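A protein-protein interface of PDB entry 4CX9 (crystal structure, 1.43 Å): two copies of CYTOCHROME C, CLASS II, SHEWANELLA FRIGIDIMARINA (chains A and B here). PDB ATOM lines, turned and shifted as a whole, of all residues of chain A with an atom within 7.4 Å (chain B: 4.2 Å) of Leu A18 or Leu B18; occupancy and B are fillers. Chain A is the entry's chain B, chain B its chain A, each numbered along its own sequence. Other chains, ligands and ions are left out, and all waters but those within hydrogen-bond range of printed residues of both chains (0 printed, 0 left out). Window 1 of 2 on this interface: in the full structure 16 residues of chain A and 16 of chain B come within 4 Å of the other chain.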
ATOM      1  N   GLU A  10     -11.634 -10.589 -18.513  1.00  0.00           N
ATOM      2  CA  GLU A  10     -12.962 -11.104 -18.137  1.00  0.00           C
ATOM      3  C   GLU A  10     -14.007  -9.980 -18.190  1.00  0.00           C
ATOM      4  O   GLU A  10     -15.133 -10.213 -18.644  1.00  0.00           O
ATOM      5  CB  GLU A  10     -12.922 -11.670 -16.715  1.00  0.00           C
ATOM      6  CG  GLU A  10     -14.267 -12.162 -16.182  1.00  0.00           C
ATOM      7  CD  GLU A  10     -14.153 -12.726 -14.777  1.00  0.00           C
ATOM      8  OE1 GLU A  10     -13.003 -13.070 -14.366  1.00  0.00           O
ATOM      9  OE2 GLU A  10     -15.200 -12.830 -14.089  1.00  0.00           O
ATOM     10  N   TYR A  11     -13.628  -8.799 -17.726  1.00  0.00           N
ATOM     11  CA  TYR A  11     -14.567  -7.631 -17.703  1.00  0.00           C
ATOM     12  C   TYR A  11     -15.044  -7.303 -19.114  1.00  0.00           C
ATOM     13  O   TYR A  11     -16.222  -7.199 -19.392  1.00  0.00           O
ATOM     14  CB  TYR A  11     -13.866  -6.448 -17.118  1.00  0.00           C
ATOM     15  CG  TYR A  11     -14.701  -5.223 -16.878  1.00  0.00           C
ATOM     16  CD1 TYR A  11     -15.519  -5.127 -15.776  1.00  0.00           C
ATOM     17  CD2 TYR A  11     -14.643  -4.129 -17.741  1.00  0.00           C
ATOM     18  CE1 TYR A  11     -16.294  -3.985 -15.550  1.00  0.00           C
ATOM     19  CE2 TYR A  11     -15.371  -2.963 -17.471  1.00  0.00           C
ATOM     20  CZ  TYR A  11     -16.194  -2.918 -16.372  1.00  0.00           C
ATOM     21  OH  TYR A  11     -16.932  -1.785 -16.078  1.00  0.00           O
ATOM     22  N   ARG A  12     -14.092  -7.160 -20.050  1.00  0.00           N
ATOM     23  CA  ARG A  12     -14.484  -6.792 -21.385  1.00  0.00           C
ATOM     24  C   ARG A  12     -15.211  -7.909 -22.157  1.00  0.00           C
ATOM     25  O   ARG A  12     -16.131  -7.639 -22.916  1.00  0.00           O
ATOM     26  CB  ARG A  12     -13.272  -6.239 -22.155  1.00  0.00           C
ATOM     27  CG  ARG A  12     -12.244  -7.298 -22.571  1.00  0.00           C
ATOM     28  CD  ARG A  12     -10.875  -6.668 -22.682  1.00  0.00           C
ATOM     29  NE  ARG A  12      -9.876  -7.562 -23.294  1.00  0.00           N
ATOM     30  CZ  ARG A  12      -8.563  -7.381 -23.156  1.00  0.00           C
ATOM     31  NH1 ARG A  12      -8.082  -6.389 -22.425  1.00  0.00           N
ATOM     32  NH2 ARG A  12      -7.726  -8.205 -23.781  1.00  0.00           N
ATOM     33  N   GLN A  13     -14.818  -9.170 -21.939  1.00  0.00           N
ATOM     34  CA  GLN A  13     -15.513 -10.308 -22.514  1.00  0.00           C
ATOM     35  C   GLN A  13     -16.954 -10.429 -21.995  1.00  0.00           C
ATOM     36  O   GLN A  13     -17.900 -10.622 -22.771  1.00  0.00           O
ATOM     37  CB  GLN A  13     -14.740 -11.612 -22.222  1.00  0.00           C
ATOM     38  CG  GLN A  13     -13.499 -11.717 -23.080  1.00  0.00           C
ATOM     39  CD  GLN A  13     -12.713 -12.987 -22.831  1.00  0.00           C
ATOM     40  OE1 GLN A  13     -12.858 -13.600 -21.777  1.00  0.00           O
ATOM     41  NE2 GLN A  13     -11.776 -13.299 -23.746  1.00  0.00           N
ATOM     42  N   ALA A  14     -17.118 -10.221 -20.697  1.00  0.00           N
ATOM     43  CA  ALA A  14     -18.464 -10.284 -20.114  1.00  0.00           C
ATOM     44  C   ALA A  14     -19.349  -9.225 -20.729  1.00  0.00           C
ATOM     45  O   ALA A  14     -20.511  -9.485 -21.136  1.00  0.00           O
ATOM     46  CB  ALA A  14     -18.402 -10.086 -18.619  1.00  0.00           C
ATOM     47  N   ALA A  15     -18.819  -8.001 -20.809  1.00  0.00           N
ATOM     48  CA  ALA A  15     -19.620  -6.914 -21.403  1.00  0.00           C
ATOM     49  C   ALA A  15     -19.992  -7.225 -22.845  1.00  0.00           C
ATOM     50  O   ALA A  15     -21.147  -7.050 -23.232  1.00  0.00           O
ATOM     51  CB  ALA A  15     -18.860  -5.607 -21.292  1.00  0.00           C
ATOM     52  N   PHE A  16     -19.035  -7.651 -23.679  1.00  0.00           N
ATOM     53  CA  PHE A  16     -19.398  -7.920 -25.060  1.00  0.00           C
ATOM     54  C   PHE A  16     -20.339  -9.097 -25.201  1.00  0.00           C
ATOM     55  O   PHE A  16     -21.158  -9.081 -26.098  1.00  0.00           O
ATOM     56  CB  PHE A  16     -18.134  -8.106 -25.909  1.00  0.00           C
ATOM     57  CG  PHE A  16     -17.529  -6.845 -26.363  1.00  0.00           C
ATOM     58  CD1 PHE A  16     -18.260  -5.927 -27.115  1.00  0.00           C
ATOM     59  CD2 PHE A  16     -16.173  -6.534 -26.088  1.00  0.00           C
ATOM     60  CE1 PHE A  16     -17.683  -4.735 -27.572  1.00  0.00           C
ATOM     61  CE2 PHE A  16     -15.640  -5.345 -26.535  1.00  0.00           C
ATOM     62  CZ  PHE A  16     -16.390  -4.457 -27.271  1.00  0.00           C
ATOM     63  N   GLY A  17     -20.238 -10.134 -24.358  1.00  0.00           N
ATOM     64  CA  GLY A  17     -21.219 -11.200 -24.392  1.00  0.00           C
ATOM     65  C   GLY A  17     -22.647 -10.742 -24.098  1.00  0.00           C
ATOM     66  O   GLY A  17     -23.592 -11.126 -24.795  1.00  0.00           O
ATOM     67  N   LEU A  18     -22.784  -9.824 -23.152  1.00  0.00           N
ATOM     68  CA  LEU A  18     -24.098  -9.233 -22.866  1.00  0.00           C
ATOM     69  C   LEU A  18     -24.578  -8.353 -24.018  1.00  0.00           C
ATOM     70  O   LEU A  18     -25.776  -8.363 -24.396  1.00  0.00           O
ATOM     71  CB  LEU A  18     -24.068  -8.424 -21.564  1.00  0.00           C
ATOM     72  CG  LEU A  18     -23.720  -9.184 -20.276  1.00  0.00           C
ATOM     73  CD1 LEU A  18     -23.639  -8.247 -19.100  1.00  0.00           C
ATOM     74  CD2 LEU A  18     -24.667 -10.332 -19.975  1.00  0.00           C
ATOM     75  N   ILE A  19     -23.655  -7.592 -24.598  1.00  0.00           N
ATOM     76  CA  ILE A  19     -23.980  -6.796 -25.777  1.00  0.00           C
ATOM     77  C   ILE A  19     -24.512  -7.680 -26.881  1.00  0.00           C
ATOM     78  O   ILE A  19     -25.522  -7.360 -27.488  1.00  0.00           O
ATOM     79  CB  ILE A  19     -22.742  -5.966 -26.237  1.00  0.00           C
ATOM     80  CG1 ILE A  19     -22.493  -4.850 -25.232  1.00  0.00           C
ATOM     81  CG2 ILE A  19     -22.928  -5.430 -27.651  1.00  0.00           C
ATOM     82  CD1 ILE A  19     -21.131  -4.165 -25.361  1.00  0.00           C
ATOM     83  N   ALA A  20     -23.809  -8.771 -27.158  1.00  0.00           N
ATOM     84  CA  ALA A  20     -24.121  -9.634 -28.338  1.00  0.00           C
ATOM     85  C   ALA A  20     -25.504 -10.288 -28.142  1.00  0.00           C
ATOM     86  O   ALA A  20     -26.273 -10.402 -29.067  1.00  0.00           O
ATOM     87  CB  ALA A  20     -23.060 -10.699 -28.442  1.00  0.00           C
ATOM     88  N   TYR A  21     -25.835 -10.644 -26.915  1.00  0.00           N
ATOM     89  CA  TYR A  21     -27.113 -11.298 -26.664  1.00  0.00           C
ATOM     90  C   TYR A  21     -28.268 -10.325 -26.913  1.00  0.00           C
ATOM     91  O   TYR A  21     -29.278 -10.640 -27.582  1.00  0.00           O
ATOM     92  CB  TYR A  21     -27.161 -11.778 -25.215  1.00  0.00           C
ATOM     93  CG  TYR A  21     -28.488 -12.398 -24.790  1.00  0.00           C
ATOM     94  CD1 TYR A  21     -28.765 -13.709 -25.040  1.00  0.00           C
ATOM     95  CD2 TYR A  21     -29.476 -11.632 -24.163  1.00  0.00           C
ATOM     96  CE1 TYR A  21     -29.981 -14.276 -24.671  1.00  0.00           C
ATOM     97  CE2 TYR A  21     -30.676 -12.180 -23.777  1.00  0.00           C
ATOM     98  CZ  TYR A  21     -30.925 -13.501 -24.028  1.00  0.00           C
ATOM     99  OH  TYR A  21     -32.147 -14.085 -23.659  1.00  0.00           O
ATOM    100  N   ASN A  22     -28.122  -9.111 -26.385  1.00  0.00           N
ATOM    101  CA  ASN A  22     -29.148  -8.104 -26.516  1.00  0.00           C
ATOM    102  C   ASN A  22     -29.250  -7.591 -27.956  1.00  0.00           C
ATOM    103  O   ASN A  22     -30.364  -7.436 -28.490  1.00  0.00           O
ATOM    104  CB  ASN A  22     -28.903  -6.972 -25.524  1.00  0.00           C
ATOM    105  CG  ASN A  22     -29.321  -7.353 -24.113  1.00  0.00           C
ATOM    106  OD1 ASN A  22     -30.518  -7.226 -23.778  1.00  0.00           O
ATOM    107  ND2 ASN A  22     -28.397  -7.879 -23.301  1.00  0.00           N
ATOM    108  N   PHE A  23     -28.094  -7.347 -28.585  1.00  0.00           N
ATOM    109  CA  PHE A  23     -28.074  -6.919 -29.972  1.00  0.00           C
ATOM    110  C   PHE A  23     -28.647  -7.994 -30.906  1.00  0.00           C
ATOM    111  O   PHE A  23     -29.398  -7.676 -31.858  1.00  0.00           O
ATOM    112  CB  PHE A  23     -26.619  -6.586 -30.355  1.00  0.00           C
ATOM    113  CG  PHE A  23     -26.504  -5.838 -31.675  1.00  0.00           C
ATOM    114  CD1 PHE A  23     -26.868  -4.528 -31.763  1.00  0.00           C
ATOM    115  CD2 PHE A  23     -26.081  -6.498 -32.801  1.00  0.00           C
ATOM    116  CE1 PHE A  23     -26.774  -3.838 -32.947  1.00  0.00           C
ATOM    117  CE2 PHE A  23     -26.015  -5.800 -34.015  1.00  0.00           C
ATOM    118  CZ  PHE A  23     -26.369  -4.498 -34.056  1.00  0.00           C
ATOM    119  N   GLY A  24     -28.344  -9.239 -30.629  1.00  0.00           N
ATOM    120  CA  GLY A  24     -28.842 -10.344 -31.476  1.00  0.00           C
ATOM    121  C   GLY A  24     -30.356 -10.469 -31.390  1.00  0.00           C
ATOM    122  O   GLY A  24     -30.992 -10.850 -32.390  1.00  0.00           O
ATOM    123  N   ARG A  44     -34.097  -3.926 -25.310  1.00  0.00           N
ATOM    124  CA  ARG A  44     -32.847  -4.424 -25.880  1.00  0.00           C
ATOM    125  C   ARG A  44     -31.937  -3.266 -26.319  1.00  0.00           C
ATOM    126  O   ARG A  44     -30.708  -3.287 -26.106  1.00  0.00           O
ATOM    127  CB  ARG A  44     -33.081  -5.335 -27.091  1.00  0.00           C
ATOM    128  CG  ARG A  44     -33.872  -6.584 -26.739  1.00  0.00           C
ATOM    129  CD  ARG A  44     -33.131  -7.440 -25.716  1.00  0.00           C
ATOM    130  NE  ARG A  44     -33.890  -8.655 -25.466  1.00  0.00           N
ATOM    131  CZ  ARG A  44     -33.693  -9.466 -24.427  1.00  0.00           C
ATOM    132  NH1 ARG A  44     -32.801  -9.179 -23.480  1.00  0.00           N
ATOM    133  NH2 ARG A  44     -34.467 -10.531 -24.282  1.00  0.00           N
ATOM    134  N   ASN A  47     -30.498  -1.479 -23.345  1.00  0.00           N
ATOM    135  CA  ASN A  47     -29.435  -2.327 -22.807  1.00  0.00           C
ATOM    136  C   ASN A  47     -28.128  -2.244 -23.628  1.00  0.00           C
ATOM    137  O   ASN A  47     -27.049  -2.090 -23.063  1.00  0.00           O
ATOM    138  CB  ASN A  47     -29.837  -3.807 -22.734  1.00  0.00           C
ATOM    139  CG  ASN A  47     -30.875  -4.104 -21.666  1.00  0.00           C
ATOM    140  OD1 ASN A  47     -31.134  -3.277 -20.773  1.00  0.00           O
ATOM    141  ND2 ASN A  47     -31.453  -5.332 -21.734  1.00  0.00           N
ATOM    142  N   VAL A  48     -28.201  -2.308 -24.951  1.00  0.00           N
ATOM    143  CA  VAL A  48     -26.988  -2.190 -25.765  1.00  0.00           C
ATOM    144  C   VAL A  48     -26.355  -0.821 -25.556  1.00  0.00           C
ATOM    145  O   VAL A  48     -25.138  -0.697 -25.454  1.00  0.00           O
ATOM    146  CB  VAL A  48     -27.239  -2.568 -27.268  1.00  0.00           C
ATOM    147  CG1 VAL A  48     -26.022  -2.201 -28.103  1.00  0.00           C
ATOM    148  CG2 VAL A  48     -27.575  -4.035 -27.392  1.00  0.00           C
ATOM    149  N   LEU A  51     -24.684  -0.820 -22.102  1.00  0.00           N
ATOM    150  CA  LEU A  51     -23.583  -1.770 -22.078  1.00  0.00           C
ATOM    151  C   LEU A  51     -22.423  -1.290 -22.941  1.00  0.00           C
ATOM    152  O   LEU A  51     -21.272  -1.572 -22.667  1.00  0.00           O
ATOM    153  CB  LEU A  51     -24.032  -3.141 -22.573  1.00  0.00           C
ATOM    154  CG  LEU A  51     -24.900  -3.951 -21.600  1.00  0.00           C
ATOM    155  CD1 LEU A  51     -25.635  -5.076 -22.344  1.00  0.00           C
ATOM    156  CD2 LEU A  51     -24.099  -4.570 -20.453  1.00  0.00           C
ATOM    157  N   ILE A  54     -19.326   0.186 -21.325  1.00  0.00           N
ATOM    158  CA  ILE A  54     -18.587  -0.652 -20.379  1.00  0.00           C
ATOM    159  C   ILE A  54     -17.225  -1.188 -20.865  1.00  0.00           C
ATOM    160  O   ILE A  54     -16.251  -1.034 -20.131  1.00  0.00           O
ATOM    161  CB  ILE A  54     -19.462  -1.832 -19.897  1.00  0.00           C
ATOM    162  CG1 ILE A  54     -20.770  -1.315 -19.293  1.00  0.00           C
ATOM    163  CG2 ILE A  54     -18.749  -2.707 -18.879  1.00  0.00           C
ATOM    164  CD1 ILE A  54     -20.587  -0.323 -18.268  1.00  0.00           C
ATOM    165  N   PRO A  55     -17.134  -1.825 -22.054  1.00  0.00           N
ATOM    166  CA  PRO A  55     -15.962  -2.698 -22.205  1.00  0.00           C
ATOM    167  C   PRO A  55     -14.664  -1.928 -22.449  1.00  0.00           C
ATOM    168  O   PRO A  55     -13.601  -2.485 -22.306  1.00  0.00           O
ATOM    169  CB  PRO A  55     -16.277  -3.513 -23.463  1.00  0.00           C
ATOM    170  CG  PRO A  55     -17.367  -2.805 -24.133  1.00  0.00           C
ATOM    171  CD  PRO A  55     -18.144  -2.070 -23.091  1.00  0.00           C
ATOM    172  N   TYR B  11     -24.830 -15.755 -18.388  1.00  0.00           N
ATOM    173  CA  TYR B  11     -25.368 -14.386 -18.630  1.00  0.00           C
ATOM    174  C   TYR B  11     -25.553 -13.633 -17.302  1.00  0.00           C
ATOM    175  O   TYR B  11     -25.056 -12.481 -17.110  1.00  0.00           O
ATOM    176  CB  TYR B  11     -26.657 -14.504 -19.410  1.00  0.00           C
ATOM    177  CG  TYR B  11     -27.339 -13.185 -19.808  1.00  0.00           C
ATOM    178  CD1 TYR B  11     -27.039 -12.575 -20.992  1.00  0.00           C
ATOM    179  CD2 TYR B  11     -28.338 -12.592 -19.000  1.00  0.00           C
ATOM    180  CE1 TYR B  11     -27.664 -11.398 -21.371  1.00  0.00           C
ATOM    181  CE2 TYR B  11     -28.938 -11.398 -19.392  1.00  0.00           C
ATOM    182  CZ  TYR B  11     -28.593 -10.823 -20.571  1.00  0.00           C
ATOM    183  OH  TYR B  11     -29.197  -9.644 -21.013  1.00  0.00           O
ATOM    184  N   ALA B  14     -22.139 -12.971 -15.581  1.00  0.00           N
ATOM    185  CA  ALA B  14     -21.409 -11.880 -16.247  1.00  0.00           C
ATOM    186  C   ALA B  14     -21.972 -10.530 -15.797  1.00  0.00           C
ATOM    187  O   ALA B  14     -21.199  -9.619 -15.498  1.00  0.00           O
ATOM    188  CB  ALA B  14     -21.495 -12.031 -17.739  1.00  0.00           C
ATOM    189  N   ALA B  15     -23.306 -10.404 -15.772  1.00  0.00           N
ATOM    190  CA  ALA B  15     -23.913  -9.113 -15.377  1.00  0.00           C
ATOM    191  C   ALA B  15     -23.562  -8.789 -13.948  1.00  0.00           C
ATOM    192  O   ALA B  15     -23.170  -7.656 -13.616  1.00  0.00           O
ATOM    193  CB  ALA B  15     -25.433  -9.146 -15.605  1.00  0.00           C
ATOM    194  N   PHE B  16     -23.676  -9.759 -13.030  1.00  0.00           N
ATOM    195  CA  PHE B  16     -23.308  -9.464 -11.658  1.00  0.00           C
ATOM    196  C   PHE B  16     -21.831  -9.081 -11.490  1.00  0.00           C
ATOM    197  O   PHE B  16     -21.491  -8.247 -10.650  1.00  0.00           O
ATOM    198  CB  PHE B  16     -23.695 -10.645 -10.704  1.00  0.00           C
ATOM    199  CG  PHE B  16     -25.172 -10.700 -10.379  1.00  0.00           C
ATOM    200  CD1 PHE B  16     -25.798  -9.625  -9.760  1.00  0.00           C
ATOM    201  CD2 PHE B  16     -25.904 -11.854 -10.653  1.00  0.00           C
ATOM    202  CE1 PHE B  16     -27.169  -9.693  -9.450  1.00  0.00           C
ATOM    203  CE2 PHE B  16     -27.251 -11.896 -10.365  1.00  0.00           C
ATOM    204  CZ  PHE B  16     -27.852 -10.814  -9.773  1.00  0.00           C
ATOM    205  N   GLY B  17     -20.930  -9.703 -12.225  1.00  0.00           N
ATOM    206  CA  GLY B  17     -19.561  -9.328 -12.168  1.00  0.00           C
ATOM    207  C   GLY B  17     -19.339  -7.878 -12.560  1.00  0.00           C
ATOM    208  O   GLY B  17     -18.569  -7.174 -11.910  1.00  0.00           O
ATOM    209  N   LEU B  18     -20.028  -7.449 -13.613  1.00  0.00           N
ATOM    210  CA  LEU B  18     -19.903  -6.026 -14.023  1.00  0.00           C
ATOM    211  C   LEU B  18     -20.544  -5.064 -13.013  1.00  0.00           C
ATOM    212  O   LEU B  18     -20.001  -3.977 -12.761  1.00  0.00           O
ATOM    213  CB  LEU B  18     -20.556  -5.820 -15.361  1.00  0.00           C
ATOM    214  CG  LEU B  18     -19.999  -6.603 -16.555  1.00  0.00           C
ATOM    215  CD1 LEU B  18     -20.829  -6.296 -17.743  1.00  0.00           C
ATOM    216  CD2 LEU B  18     -18.553  -6.217 -16.777  1.00  0.00           C
ATOM    217  N   ILE B  19     -21.645  -5.495 -12.402  1.00  0.00           N
ATOM    218  CA  ILE B  19     -22.240  -4.722 -11.310  1.00  0.00           C
ATOM    219  C   ILE B  19     -21.225  -4.594 -10.202  1.00  0.00           C
ATOM    220  O   ILE B  19     -21.018  -3.495  -9.652  1.00  0.00           O
ATOM    221  CB  ILE B  19     -23.523  -5.417 -10.814  1.00  0.00           C
ATOM    222  CG1 ILE B  19     -24.617  -5.236 -11.842  1.00  0.00           C
ATOM    223  CG2 ILE B  19     -23.949  -4.859  -9.479  1.00  0.00           C
ATOM    224  CD1 ILE B  19     -25.838  -6.112 -11.610  1.00  0.00           C
ATOM    225  N   ALA B  20     -20.594  -5.690  -9.807  1.00  0.00           N
ATOM    226  CA  ALA B  20     -19.700  -5.662  -8.652  1.00  0.00           C
ATOM    227  C   ALA B  20     -18.463  -4.784  -8.892  1.00  0.00           C
ATOM    228  O   ALA B  20     -17.977  -4.106  -7.982  1.00  0.00           O
ATOM    229  CB  ALA B  20     -19.285  -7.052  -8.279  1.00  0.00           C
ATOM    230  N   TYR B  21     -17.953  -4.813 -10.099  1.00  0.00           N
ATOM    231  CA  TYR B  21     -16.774  -3.985 -10.434  1.00  0.00           C
ATOM    232  C   TYR B  21     -17.131  -2.479 -10.268  1.00  0.00           C
ATOM    233  O   TYR B  21     -16.399  -1.700  -9.677  1.00  0.00           O
ATOM    234  CB  TYR B  21     -16.296  -4.267 -11.863  1.00  0.00           C
ATOM    235  CG  TYR B  21     -15.154  -3.378 -12.301  1.00  0.00           C
ATOM    236  CD1 TYR B  21     -13.848  -3.716 -12.003  1.00  0.00           C
ATOM    237  CD2 TYR B  21     -15.434  -2.154 -12.930  1.00  0.00           C
ATOM    238  CE1 TYR B  21     -12.803  -2.856 -12.327  1.00  0.00           C
ATOM    239  CE2 TYR B  21     -14.398  -1.288 -13.308  1.00  0.00           C
ATOM    240  CZ  TYR B  21     -13.090  -1.681 -13.009  1.00  0.00           C
ATOM    241  OH  TYR B  21     -11.976  -0.897 -13.334  1.00  0.00           O
ATOM    242  N   ASN B  22     -18.261  -2.084 -10.848  1.00  0.00           N
ATOM    243  CA  ASN B  22     -18.690  -0.691 -10.794  1.00  0.00           C
ATOM    244  C   ASN B  22     -19.092  -0.254  -9.400  1.00  0.00           C
ATOM    245  O   ASN B  22     -18.674   0.811  -8.932  1.00  0.00           O
ATOM    246  CB  ASN B  22     -19.789  -0.484 -11.819  1.00  0.00           C
ATOM    247  CG  ASN B  22     -19.241  -0.346 -13.223  1.00  0.00           C
ATOM    248  OD1 ASN B  22     -18.775   0.750 -13.624  1.00  0.00           O
ATOM    249  ND2 ASN B  22     -19.168  -1.463 -13.955  1.00  0.00           N
ATOM    250  N   LEU B  51     -27.174  -1.798 -15.379  1.00  0.00           N
ATOM    251  CA  LEU B  51     -26.831  -3.171 -15.263  1.00  0.00           C
ATOM    252  C   LEU B  51     -27.779  -3.930 -14.350  1.00  0.00           C
ATOM    253  O   LEU B  51     -27.973  -5.145 -14.542  1.00  0.00           O
ATOM    254  CB  LEU B  51     -25.425  -3.318 -14.757  1.00  0.00           C
ATOM    255  CG  LEU B  51     -24.282  -2.974 -15.705  1.00  0.00           C
ATOM    256  CD1 LEU B  51     -22.950  -2.787 -14.985  1.00  0.00           C
ATOM    257  CD2 LEU B  51     -24.127  -4.023 -16.815  1.00  0.00           C
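Of the printed residues of chain B, Ala A15 touches Leu B18 (3.9 Å). Printed residues of chain B within 4 Å of Asn A22: Tyr B11 (3.0 Å). Of the printed residues of chain B, Leu A51 touches Leu B51. Of chain A, only Tyr A11 (3.4 Å), Ala A15 (3.9 Å) and Leu A18 (3.7 Å) come within 4 Å of Leu B18. Printed residues of chain A within 4 Å of Tyr B21: Tyr A11 (3.3 Å). Of the printed residues of chain A, Leu B51 touches Leu A51 (3.7 Å). The nearest printed residue of chain A that does not touch Tyr B21 is Ile A54 (6.8 Å).
Of the 21 printed residues of chain A, 7 touch a printed residue of chain B. Printed residues of chain A that touch a printed residue of chain B: Tyr A11, Ala A14, Ala A15, Leu A18, Tyr A21, Asn A22 and Leu A51. Hydrophobic or aromatic side chains of chain A within 4 Å of the printed part of chain B: Tyr A11, Ala A14, Leu A18, Tyr A21 and Leu A51. Along chain A the printed residues that touch a printed residue of chain B span positions 11 to 51. Of the 11 printed residues of chain B, 7 touch a printed residue of chain A. Printed residues of chain B that touch a printed residue of chain A: Tyr B11, Ala B14, Ala B15, Leu B18, Tyr B21, Asn B22 and Leu B51. Among the printed residues, 11 pairs touch across the chains. Among the printed residues, no Asp or Glu carboxylate lies within 4 Å of a Lys or Arg side-chain nitrogen of the other chain.
CD1 of Tyr A11 touches CD2 of Leu B18 (3.4 Å). Tyr B21 touches Tyr A11 (CD2 to CE1, 3.3 Å). Ala A14 touches Ala B14. Leu B18 touches Ala A15. CD1 of Tyr B11 touches CD2 of Leu A18, 3.4 Å away. CD1 of Leu A18 touches CA of Ala B15 (3.8 Å). Leu A18 touches Leu B18 (CD1 to CD1, 3.7 Å). CE1 of Tyr B11 touches CD2 of Tyr A21, 3.3 Å away. Leu A51 touches Leu B51.
Tyr A11 touches Leu B18, and with the chains exchanged Leu A18 touches Tyr B11. Tyr A11 touches Tyr B21, and with the chains exchanged Tyr A21 touches Tyr B11. Leu B18 touches its own counterpart, Leu A18. Leu A51 touches its own counterpart, Leu B51. Positions printed for both chains: 11, 14, 15, 16, 17, 18, 19, 20, 21, 22 and 51.
The side-chain amide nitrogen of Asn A22 lies within hydrogen-bond range of the side-chain hydroxyl of Tyr B11. ND2 of Asn B22 is in hydrogen-bond range of OH of Tyr A11, at 3.1 Å.
The backbone carbonyl oxygen (O) of Leu B18 is in hydrogen-bond range of the side-chain amide nitrogen (ND2) of Asn B22 (2.9 Å). ND2 of Asn A22 sits at hydrogen-bond distance from O of Leu A18, at 2.9 Å. The side-chain amide oxygen (OD1) of Asn A22 is in hydrogen-bond range of the guanidinium group (NH1) of Arg A44, 3.0 Å away. The side-chain amide nitrogen of Asn A47 sits at hydrogen-bond distance from the side-chain amide oxygen of Asn A22, at 2.9 Å.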
